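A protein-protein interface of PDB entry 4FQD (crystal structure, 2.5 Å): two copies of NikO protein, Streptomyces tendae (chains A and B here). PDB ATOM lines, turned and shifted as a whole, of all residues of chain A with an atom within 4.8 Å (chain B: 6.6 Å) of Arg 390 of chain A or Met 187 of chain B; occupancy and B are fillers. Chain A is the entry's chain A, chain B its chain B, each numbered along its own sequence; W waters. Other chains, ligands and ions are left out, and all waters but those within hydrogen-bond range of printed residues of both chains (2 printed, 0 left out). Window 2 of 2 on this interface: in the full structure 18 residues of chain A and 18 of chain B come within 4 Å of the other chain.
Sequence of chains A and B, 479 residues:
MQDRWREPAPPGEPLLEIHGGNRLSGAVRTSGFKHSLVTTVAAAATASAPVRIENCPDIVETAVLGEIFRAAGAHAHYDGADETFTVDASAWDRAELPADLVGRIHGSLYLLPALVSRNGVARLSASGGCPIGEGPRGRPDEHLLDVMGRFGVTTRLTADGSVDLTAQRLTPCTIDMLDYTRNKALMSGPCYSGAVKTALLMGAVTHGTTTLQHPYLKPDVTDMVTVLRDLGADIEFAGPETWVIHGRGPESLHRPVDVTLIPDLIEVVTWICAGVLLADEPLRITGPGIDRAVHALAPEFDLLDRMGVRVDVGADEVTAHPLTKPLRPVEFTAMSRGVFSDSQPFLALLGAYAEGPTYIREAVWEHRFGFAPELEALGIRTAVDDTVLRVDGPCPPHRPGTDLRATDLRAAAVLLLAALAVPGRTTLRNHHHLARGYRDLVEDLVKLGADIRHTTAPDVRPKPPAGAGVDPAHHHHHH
N of Arg 390 of chain A lies within hydrogen-bond range of O of Ala 383 of chain A, 2.8 Å away.
The backbone NH (N) of Ala 185 of chain B sits at hydrogen-bond distance from the side-chain amide oxygen (OD1) of Asn 183 of chain B, at 3.2 Å.
OD1 of Asn 183 of chain B lies within hydrogen-bond range of N of Leu 186 of chain B, at 2.8 Å.
N of Asn 183 of chain B is in hydrogen-bond range of O of Ser 188 of chain B.
SD of Met 187 of chain B sits close to NH1 of Arg 337 of chain B.
NH2 of Arg 337 of chain B sits at hydrogen-bond distance from OH of Tyr 192 of chain B (3.4 Å).
Water W2 lies within hydrogen-bond range of OH of Tyr 359 of chain A (2.4 Å) and NH1 of Arg 337 of chain B (3.2 Å).
Water W1 lies within hydrogen-bond range of O of Arg 337 of chain B and OH of Tyr 359 of chain A.
CD2 of Tyr 359 of chain A touches CD1 of Leu 186 of chain B, at 3.6 Å.
Tyr 359 of chain A touches Met 335 of chain B.
OH of Tyr 359 of chain A touches CB of Arg 337 of chain B, 3.8 Å away.
Ala 185 of chain B touches Ala 383 of chain A (CB to O, 3.5 Å).
Asn 183 of chain B touches Val 388 of chain A.
Val 388 of chain A touches Ala 185 of chain B (O to CB, 3.5 Å).
N of Leu 186 of chain B touches CG1 of Val 388 of chain A, 3.7 Å away.
The guanidinium group (NH2) of Arg 390 of chain A is in hydrogen-bond range of the backbone carbonyl oxygen (O) of Lys 184 of chain B (3.1 Å).
NE of Arg 390 of chain A sits at hydrogen-bond distance from O of Ala 185 of chain B.
NH2 of Arg 390 of chain A sits close to SD of Met 187 of chain B (3.5 Å).
No position is printed for both chains.
Of the 10 pairs that touch across the chains among the printed residues, none has its exchanged pair printed and touching as well.
Of the 18 printed residues of chain B, 7 touch a printed residue of chain A.
Hydrophobic or aromatic side chains of chain B that line the printed part of chain A: Ala 185, Leu 186, Met 187 and Met 335.
Of the 11 printed residues of chain A, 4 touch a printed residue of chain B.
Printed residues of chain A that touch a printed residue of chain B: Tyr 359, Ala 383, Val 388 and Arg 390.
Along chain A the printed residues that touch a printed residue of chain B span positions 359 to 390.
Among the printed residues, 10 pairs touch across the chains.
Among the printed residues, no Asp or Glu carboxylate lies within 4 Å of a Lys or Arg side-chain nitrogen of the other chain.
Printed residues of chain B within 4 Å of Tyr 359 of chain A: Leu 186 (3.6 Å), Met 335 (3.7 Å) and Arg 337 (3.8 Å).
Of the printed residues of chain B, Val 388 of chain A touches Asn 183, Ala 185 and Leu 186.
Arg 390 of chain A touches three residues of chain B.
Leu 178 of chain B touches none of the printed residues of chain A.
Printed residues of chain A within 4 Å of Leu 186 of chain B: Tyr 359 (3.6 Å) and Val 388 (3.7 Å).
Of the printed residues of chain A, Met 187 of chain B touches Arg 390.
Tyr 216 of chain B touches none of the printed residues of chain A.
Of the printed residues of chain A, Met 335 of chain B touches Tyr 359.
Of the printed residues of chain A, Arg 337 of chain B touches Tyr 359.
The nearest printed residue of chain A that does not touch Met 187 of chain B is Tyr 359 of chain A (4.8 Å).
The nearest printed residue of chain B that does not touch Val 388 of chain A is Met 187 of chain B (6.2 Å).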
ATOM      1  N   PRO A 357      16.533  13.025  -9.026  1.00  0.00           N
ATOM      2  CA  PRO A 357      17.235  13.266  -7.763  1.00  0.00           C
ATOM      3  C   PRO A 357      18.516  14.070  -7.961  1.00  0.00           C
ATOM      4  O   PRO A 357      19.333  13.724  -8.813  1.00  0.00           O
ATOM      5  CB  PRO A 357      17.595  11.852  -7.280  1.00  0.00           C
ATOM      6  CG  PRO A 357      16.931  10.896  -8.247  1.00  0.00           C
ATOM      7  CD  PRO A 357      16.745  11.653  -9.512  1.00  0.00           C
ATOM      8  N   THR A 358      18.681  15.133  -7.181  1.00  0.00           N
ATOM      9  CA  THR A 358      19.933  15.880  -7.167  1.00  0.00           C
ATOM     10  C   THR A 358      20.709  15.551  -5.898  1.00  0.00           C
ATOM     11  O   THR A 358      20.204  15.724  -4.790  1.00  0.00           O
ATOM     12  CB  THR A 358      19.698  17.401  -7.248  1.00  0.00           C
ATOM     13  OG1 THR A 358      19.320  17.756  -8.584  1.00  0.00           O
ATOM     14  CG2 THR A 358      20.966  18.157  -6.878  1.00  0.00           C
ATOM     15  N   TYR A 359      21.936  15.069  -6.065  1.00  0.00           N
ATOM     16  CA  TYR A 359      22.764  14.676  -4.932  1.00  0.00           C
ATOM     17  C   TYR A 359      23.855  15.705  -4.670  1.00  0.00           C
ATOM     18  O   TYR A 359      24.681  15.984  -5.538  1.00  0.00           O
ATOM     19  CB  TYR A 359      23.384  13.298  -5.173  1.00  0.00           C
ATOM     20  CG  TYR A 359      22.371  12.212  -5.453  1.00  0.00           C
ATOM     21  CD1 TYR A 359      21.939  11.956  -6.749  1.00  0.00           C
ATOM     22  CD2 TYR A 359      21.846  11.443  -4.424  1.00  0.00           C
ATOM     23  CE1 TYR A 359      21.014  10.965  -7.011  1.00  0.00           C
ATOM     24  CE2 TYR A 359      20.919  10.448  -4.675  1.00  0.00           C
ATOM     25  CZ  TYR A 359      20.507  10.214  -5.971  1.00  0.00           C
ATOM     26  OH  TYR A 359      19.585   9.225  -6.228  1.00  0.00           O
ATOM     27  N   ARG A 381      11.082  18.677  -1.408  1.00  0.00           N
ATOM     28  CA  ARG A 381      11.424  17.399  -0.791  1.00  0.00           C
ATOM     29  C   ARG A 381      12.935  17.233  -0.669  1.00  0.00           C
ATOM     30  O   ARG A 381      13.640  17.168  -1.676  1.00  0.00           O
ATOM     31  CB  ARG A 381      10.860  16.245  -1.621  1.00  0.00           C
ATOM     32  CG  ARG A 381       9.410  16.413  -2.045  1.00  0.00           C
ATOM     33  CD  ARG A 381       8.446  15.888  -0.999  1.00  0.00           C
ATOM     34  NE  ARG A 381       7.240  15.343  -1.614  1.00  0.00           N
ATOM     35  CZ  ARG A 381       6.177  16.067  -1.951  1.00  0.00           C
ATOM     36  NH1 ARG A 381       6.167  17.374  -1.732  1.00  0.00           N
ATOM     37  NH2 ARG A 381       5.126  15.484  -2.509  1.00  0.00           N
ATOM     38  N   THR A 382      13.431  17.159   0.562  1.00  0.00           N
ATOM     39  CA  THR A 382      14.861  16.983   0.792  1.00  0.00           C
ATOM     40  C   THR A 382      15.157  15.814   1.727  1.00  0.00           C
ATOM     41  O   THR A 382      14.277  15.329   2.437  1.00  0.00           O
ATOM     42  CB  THR A 382      15.512  18.251   1.381  1.00  0.00           C
ATOM     43  OG1 THR A 382      15.002  18.485   2.699  1.00  0.00           O
ATOM     44  CG2 THR A 382      15.234  19.465   0.502  1.00  0.00           C
ATOM     45  N   ALA A 383      16.409  15.369   1.712  1.00  0.00           N
ATOM     46  CA  ALA A 383      16.881  14.335   2.624  1.00  0.00           C
ATOM     47  C   ALA A 383      18.330  14.627   2.992  1.00  0.00           C
ATOM     48  O   ALA A 383      19.150  14.921   2.122  1.00  0.00           O
ATOM     49  CB  ALA A 383      16.752  12.960   1.992  1.00  0.00           C
ATOM     50  N   VAL A 388      25.785  14.629   3.126  1.00  0.00           N
ATOM     51  CA  VAL A 388      25.039  14.499   1.880  1.00  0.00           C
ATOM     52  C   VAL A 388      23.636  15.088   1.959  1.00  0.00           C
ATOM     53  O   VAL A 388      22.896  14.835   2.909  1.00  0.00           O
ATOM     54  CB  VAL A 388      24.951  13.021   1.438  1.00  0.00           C
ATOM     55  CG1 VAL A 388      24.065  12.873   0.205  1.00  0.00           C
ATOM     56  CG2 VAL A 388      26.341  12.470   1.171  1.00  0.00           C
ATOM     57  N   LEU A 389      23.285  15.881   0.952  1.00  0.00           N
ATOM     58  CA  LEU A 389      21.931  16.396   0.802  1.00  0.00           C
ATOM     59  C   LEU A 389      21.348  15.936  -0.529  1.00  0.00           C
ATOM     60  O   LEU A 389      22.004  16.026  -1.568  1.00  0.00           O
ATOM     61  CB  LEU A 389      21.927  17.924   0.874  1.00  0.00           C
ATOM     62  CG  LEU A 389      20.671  18.631   0.358  1.00  0.00           C
ATOM     63  CD1 LEU A 389      19.456  18.276   1.203  1.00  0.00           C
ATOM     64  CD2 LEU A 389      20.884  20.138   0.319  1.00  0.00           C
ATOM     65  N   ARG A 390      20.117  15.438  -0.494  1.00  0.00           N
ATOM     66  CA  ARG A 390      19.451  14.984  -1.708  1.00  0.00           C
ATOM     67  C   ARG A 390      18.140  15.731  -1.919  1.00  0.00           C
ATOM     68  O   ARG A 390      17.367  15.923  -0.982  1.00  0.00           O
ATOM     69  CB  ARG A 390      19.192  13.478  -1.649  1.00  0.00           C
ATOM     70  CG  ARG A 390      18.705  12.879  -2.959  1.00  0.00           C
ATOM     71  CD  ARG A 390      17.505  11.979  -2.728  1.00  0.00           C
ATOM     72  NE  ARG A 390      17.717  11.061  -1.613  1.00  0.00           N
ATOM     73  CZ  ARG A 390      16.756  10.638  -0.799  1.00  0.00           C
ATOM     74  NH1 ARG A 390      15.508  11.053  -0.972  1.00  0.00           N
ATOM     75  NH2 ARG A 390      17.041   9.804   0.191  1.00  0.00           N
ATOM     76  N   VAL A 391      17.899  16.157  -3.154  1.00  0.00           N
ATOM     77  CA  VAL A 391      16.652  16.820  -3.509  1.00  0.00           C
ATOM     78  C   VAL A 391      15.863  15.971  -4.500  1.00  0.00           C
ATOM     79  O   VAL A 391      16.366  15.620  -5.568  1.00  0.00           O
ATOM     80  CB  VAL A 391      16.903  18.219  -4.110  1.00  0.00           C
ATOM     81  CG1 VAL A 391      15.595  18.844  -4.570  1.00  0.00           C
ATOM     82  CG2 VAL A 391      17.599  19.113  -3.096  1.00  0.00           C
ATOM     83  N   ASP A 392      14.627  15.640  -4.139  1.00  0.00           N
ATOM     84  CA  ASP A 392      13.779  14.802  -4.980  1.00  0.00           C
ATOM     85  C   ASP A 392      12.925  15.628  -5.935  1.00  0.00           C
ATOM     86  O   ASP A 392      11.739  15.845  -5.690  1.00  0.00           O
ATOM     87  CB  ASP A 392      12.882  13.911  -4.119  1.00  0.00           C
ATOM     88  CG  ASP A 392      13.658  12.829  -3.399  1.00  0.00           C
ATOM     89  OD1 ASP A 392      14.634  12.312  -3.981  1.00  0.00           O
ATOM     90  OD2 ASP A 392      13.292  12.494  -2.253  1.00  0.00           O
ATOM     91  N   LEU B 178      16.419   1.505   3.074  1.00  0.00           N
ATOM     92  CA  LEU B 178      17.429   2.482   3.465  1.00  0.00           C
ATOM     93  C   LEU B 178      18.118   2.076   4.763  1.00  0.00           C
ATOM     94  O   LEU B 178      19.127   2.663   5.152  1.00  0.00           O
ATOM     95  CB  LEU B 178      16.814   3.876   3.605  1.00  0.00           C
ATOM     96  CG  LEU B 178      16.353   4.535   2.303  1.00  0.00           C
ATOM     97  CD1 LEU B 178      15.934   5.977   2.549  1.00  0.00           C
ATOM     98  CD2 LEU B 178      17.446   4.460   1.247  1.00  0.00           C
ATOM     99  N   THR B 181      21.661   0.852   3.863  1.00  0.00           N
ATOM    100  CA  THR B 181      22.559   1.766   3.168  1.00  0.00           C
ATOM    101  C   THR B 181      23.490   2.440   4.169  1.00  0.00           C
ATOM    102  O   THR B 181      23.153   2.574   5.346  1.00  0.00           O
ATOM    103  CB  THR B 181      21.782   2.854   2.402  1.00  0.00           C
ATOM    104  OG1 THR B 181      21.034   3.654   3.328  1.00  0.00           O
ATOM    105  CG2 THR B 181      20.831   2.226   1.393  1.00  0.00           C
ATOM    106  N   ARG B 182      24.662   2.857   3.704  1.00  0.00           N
ATOM    107  CA  ARG B 182      25.594   3.586   4.556  1.00  0.00           C
ATOM    108  C   ARG B 182      25.131   5.028   4.723  1.00  0.00           C
ATOM    109  O   ARG B 182      25.099   5.555   5.834  1.00  0.00           O
ATOM    110  CB  ARG B 182      27.011   3.550   3.983  1.00  0.00           C
ATOM    111  CG  ARG B 182      28.016   4.334   4.811  1.00  0.00           C
ATOM    112  CD  ARG B 182      29.391   4.372   4.162  1.00  0.00           C
ATOM    113  NE  ARG B 182      30.029   3.060   4.128  1.00  0.00           N
ATOM    114  CZ  ARG B 182      30.235   2.357   3.018  1.00  0.00           C
ATOM    115  NH1 ARG B 182      29.857   2.842   1.844  1.00  0.00           N
ATOM    116  NH2 ARG B 182      30.824   1.170   3.083  1.00  0.00           N
ATOM    117  N   ASN B 183      24.775   5.660   3.611  1.00  0.00           N
ATOM    118  CA  ASN B 183      24.235   7.013   3.635  1.00  0.00           C
ATOM    119  C   ASN B 183      22.807   7.034   3.099  1.00  0.00           C
ATOM    120  O   ASN B 183      22.569   6.738   1.928  1.00  0.00           O
ATOM    121  CB  ASN B 183      25.119   7.965   2.831  1.00  0.00           C
ATOM    122  CG  ASN B 183      24.758   9.422   3.051  1.00  0.00           C
ATOM    123  OD1 ASN B 183      23.805   9.933   2.465  1.00  0.00           O
ATOM    124  ND2 ASN B 183      25.523  10.098   3.902  1.00  0.00           N
ATOM    125  N   LYS B 184      21.862   7.386   3.965  1.00  0.00           N
ATOM    126  CA  LYS B 184      20.444   7.320   3.627  1.00  0.00           C
ATOM    127  C   LYS B 184      19.990   8.412   2.660  1.00  0.00           C
ATOM    128  O   LYS B 184      19.045   8.218   1.896  1.00  0.00           O
ATOM    129  CB  LYS B 184      19.601   7.331   4.903  1.00  0.00           C
ATOM    130  CG  LYS B 184      19.717   6.038   5.693  1.00  0.00           C
ATOM    131  CD  LYS B 184      19.390   6.227   7.159  1.00  0.00           C
ATOM    132  CE  LYS B 184      19.429   4.895   7.894  1.00  0.00           C
ATOM    133  NZ  LYS B 184      20.659   4.119   7.573  1.00  0.00           N
ATOM    134  N   ALA B 185      20.666   9.555   2.690  1.00  0.00           N
ATOM    135  CA  ALA B 185      20.364  10.632   1.756  1.00  0.00           C
ATOM    136  C   ALA B 185      20.843  10.258   0.360  1.00  0.00           C
ATOM    137  O   ALA B 185      20.133  10.451  -0.627  1.00  0.00           O
ATOM    138  CB  ALA B 185      21.006  11.933   2.209  1.00  0.00           C
ATOM    139  N   LEU B 186      22.053   9.710   0.287  1.00  0.00           N
ATOM    140  CA  LEU B 186      22.635   9.305  -0.985  1.00  0.00           C
ATOM    141  C   LEU B 186      22.017   7.997  -1.464  1.00  0.00           C
ATOM    142  O   LEU B 186      22.079   7.670  -2.650  1.00  0.00           O
ATOM    143  CB  LEU B 186      24.151   9.147  -0.854  1.00  0.00           C
ATOM    144  CG  LEU B 186      24.943   9.188  -2.162  1.00  0.00           C
ATOM    145  CD1 LEU B 186      24.921  10.592  -2.753  1.00  0.00           C
ATOM    146  CD2 LEU B 186      26.370   8.710  -1.952  1.00  0.00           C
ATOM    147  N   MET B 187      21.420   7.263  -0.527  1.00  0.00           N
ATOM    148  CA  MET B 187      20.813   5.962  -0.800  1.00  0.00           C
ATOM    149  C   MET B 187      21.834   5.007  -1.407  1.00  0.00           C
ATOM    150  O   MET B 187      21.601   4.420  -2.464  1.00  0.00           O
ATOM    151  CB  MET B 187      19.593   6.106  -1.715  1.00  0.00           C
ATOM    152  CG  MET B 187      18.658   7.239  -1.320  1.00  0.00           C
ATOM    153  SD  MET B 187      17.230   7.407  -2.407  1.00  0.00           S
ATOM    154  CE  MET B 187      16.142   6.155  -1.741  1.00  0.00           C
ATOM    155  N   SER B 188      22.968   4.861  -0.729  1.00  0.00           N
ATOM    156  CA  SER B 188      24.062   4.040  -1.232  1.00  0.00           C
ATOM    157  C   SER B 188      24.720   3.236  -0.115  1.00  0.00           C
ATOM    158  O   SER B 188      24.749   3.664   1.040  1.00  0.00           O
ATOM    159  CB  SER B 188      25.102   4.919  -1.932  1.00  0.00           C
ATOM    160  OG  SER B 188      26.145   4.138  -2.487  1.00  0.00           O
ATOM    161  N   GLY B 189      25.250   2.069  -0.470  1.00  0.00           N
ATOM    162  CA  GLY B 189      25.908   1.202   0.490  1.00  0.00           C
ATOM    163  C   GLY B 189      26.183  -0.177  -0.078  1.00  0.00           C
ATOM    164  O   GLY B 189      25.550  -0.588  -1.050  1.00  0.00           O
ATOM    165  N   TYR B 192      23.140  -2.570   0.365  1.00  0.00           N
ATOM    166  CA  TYR B 192      21.902  -2.107  -0.255  1.00  0.00           C
ATOM    167  C   TYR B 192      21.363  -3.104  -1.278  1.00  0.00           C
ATOM    168  O   TYR B 192      20.228  -3.571  -1.167  1.00  0.00           O
ATOM    169  CB  TYR B 192      22.144  -0.751  -0.923  1.00  0.00           C
ATOM    170  CG  TYR B 192      20.899  -0.020  -1.384  1.00  0.00           C
ATOM    171  CD1 TYR B 192      19.636  -0.390  -0.940  1.00  0.00           C
ATOM    172  CD2 TYR B 192      20.994   1.045  -2.268  1.00  0.00           C
ATOM    173  CE1 TYR B 192      18.504   0.282  -1.365  1.00  0.00           C
ATOM    174  CE2 TYR B 192      19.872   1.723  -2.698  1.00  0.00           C
ATOM    175  CZ  TYR B 192      18.630   1.339  -2.245  1.00  0.00           C
ATOM    176  OH  TYR B 192      17.517   2.017  -2.679  1.00  0.00           O
ATOM    177  N   HIS B 214      12.032   2.207  -1.005  1.00  0.00           N
ATOM    178  CA  HIS B 214      13.319   2.682  -1.512  1.00  0.00           C
ATOM    179  C   HIS B 214      14.210   1.537  -1.992  1.00  0.00           C
ATOM    180  O   HIS B 214      15.294   1.323  -1.448  1.00  0.00           O
ATOM    181  CB  HIS B 214      14.045   3.508  -0.447  1.00  0.00           C
ATOM    182  CG  HIS B 214      13.237   4.648   0.088  1.00  0.00           C
ATOM    183  ND1 HIS B 214      12.753   4.676   1.379  1.00  0.00           N
ATOM    184  CD2 HIS B 214      12.823   5.799  -0.494  1.00  0.00           C
ATOM    185  CE1 HIS B 214      12.080   5.796   1.570  1.00  0.00           C
ATOM    186  NE2 HIS B 214      12.106   6.494   0.450  1.00  0.00           N
ATOM    187  N   PRO B 215      13.758   0.801  -3.019  1.00  0.00           N
ATOM    188  CA  PRO B 215      14.494  -0.385  -3.460  1.00  0.00           C
ATOM    189  C   PRO B 215      15.607  -0.060  -4.452  1.00  0.00           C
ATOM    190  O   PRO B 215      15.594   0.998  -5.081  1.00  0.00           O
ATOM    191  CB  PRO B 215      13.412  -1.209  -4.154  1.00  0.00           C
ATOM    192  CG  PRO B 215      12.517  -0.179  -4.754  1.00  0.00           C
ATOM    193  CD  PRO B 215      12.531   1.005  -3.812  1.00  0.00           C
ATOM    194  N   TYR B 216      16.562  -0.978  -4.572  1.00  0.00           N
ATOM    195  CA  TYR B 216      17.628  -0.891  -5.560  1.00  0.00           C
ATOM    196  C   TYR B 216      16.987  -0.924  -6.945  1.00  0.00           C
ATOM    197  O   TYR B 216      16.010  -1.641  -7.158  1.00  0.00           O
ATOM    198  CB  TYR B 216      18.584  -2.068  -5.370  1.00  0.00           C
ATOM    199  CG  TYR B 216      19.902  -1.960  -6.099  1.00  0.00           C
ATOM    200  CD1 TYR B 216      20.866  -1.040  -5.705  1.00  0.00           C
ATOM    201  CD2 TYR B 216      20.199  -2.804  -7.161  1.00  0.00           C
ATOM    202  CE1 TYR B 216      22.080  -0.950  -6.364  1.00  0.00           C
ATOM    203  CE2 TYR B 216      21.406  -2.724  -7.823  1.00  0.00           C
ATOM    204  CZ  TYR B 216      22.344  -1.797  -7.422  1.00  0.00           C
ATOM    205  OH  TYR B 216      23.544  -1.722  -8.089  1.00  0.00           O
ATOM    206  N   GLU B 241       8.962   4.587  -5.126  1.00  0.00           N
ATOM    207  CA  GLU B 241       9.805   4.088  -4.048  1.00  0.00           C
ATOM    208  C   GLU B 241       9.082   3.040  -3.209  1.00  0.00           C
ATOM    209  O   GLU B 241       9.483   2.756  -2.082  1.00  0.00           O
ATOM    210  CB  GLU B 241      10.256   5.241  -3.147  1.00  0.00           C
ATOM    211  CG  GLU B 241      10.955   6.380  -3.877  1.00  0.00           C
ATOM    212  CD  GLU B 241      12.337   6.002  -4.375  1.00  0.00           C
ATOM    213  OE1 GLU B 241      12.834   4.921  -3.995  1.00  0.00           O
ATOM    214  OE2 GLU B 241      12.929   6.789  -5.142  1.00  0.00           O
ATOM    215  N   MET B 335      28.088   5.404  -6.738  1.00  0.00           N
ATOM    216  CA  MET B 335      27.059   5.118  -5.747  1.00  0.00           C
ATOM    217  C   MET B 335      26.021   4.125  -6.261  1.00  0.00           C
ATOM    218  O   MET B 335      25.983   3.807  -7.450  1.00  0.00           O
ATOM    219  CB  MET B 335      26.378   6.414  -5.307  1.00  0.00           C
ATOM    220  CG  MET B 335      25.809   7.224  -6.456  1.00  0.00           C
ATOM    221  SD  MET B 335      25.211   8.842  -5.941  1.00  0.00           S
ATOM    222  CE  MET B 335      24.480   9.424  -7.469  1.00  0.00           C
ATOM    223  N   SER B 336      25.176   3.651  -5.351  1.00  0.00           N
ATOM    224  CA  SER B 336      24.192   2.617  -5.657  1.00  0.00           C
ATOM    225  C   SER B 336      23.161   3.061  -6.690  1.00  0.00           C
ATOM    226  O   SER B 336      22.818   2.303  -7.598  1.00  0.00           O
ATOM    227  CB  SER B 336      23.486   2.162  -4.377  1.00  0.00           C
ATOM    228  OG  SER B 336      24.404   1.602  -3.453  1.00  0.00           O
ATOM    229  N   ARG B 337      22.662   4.284  -6.547  1.00  0.00           N
ATOM    230  CA  ARG B 337      21.700   4.825  -7.501  1.00  0.00           C
ATOM    231  C   ARG B 337      22.386   5.737  -8.511  1.00  0.00           C
ATOM    232  O   ARG B 337      21.788   6.689  -9.013  1.00  0.00           O
ATOM    233  CB  ARG B 337      20.575   5.571  -6.782  1.00  0.00           C
ATOM    234  CG  ARG B 337      19.651   4.665  -5.987  1.00  0.00           C
ATOM    235  CD  ARG B 337      18.332   5.354  -5.683  1.00  0.00           C
ATOM    236  NE  ARG B 337      17.354   4.431  -5.116  1.00  0.00           N
ATOM    237  CZ  ARG B 337      16.077   4.732  -4.910  1.00  0.00           C
ATOM    238  NH1 ARG B 337      15.621   5.937  -5.224  1.00  0.00           N
ATOM    239  NH2 ARG B 337      15.256   3.830  -4.390  1.00  0.00           N
HETATM  240  O   HOH W   1      19.639   8.516  -8.975  1.00  0.00           O
HETATM  241  O   HOH W   2      17.271   8.519  -6.133  1.00  0.00           O
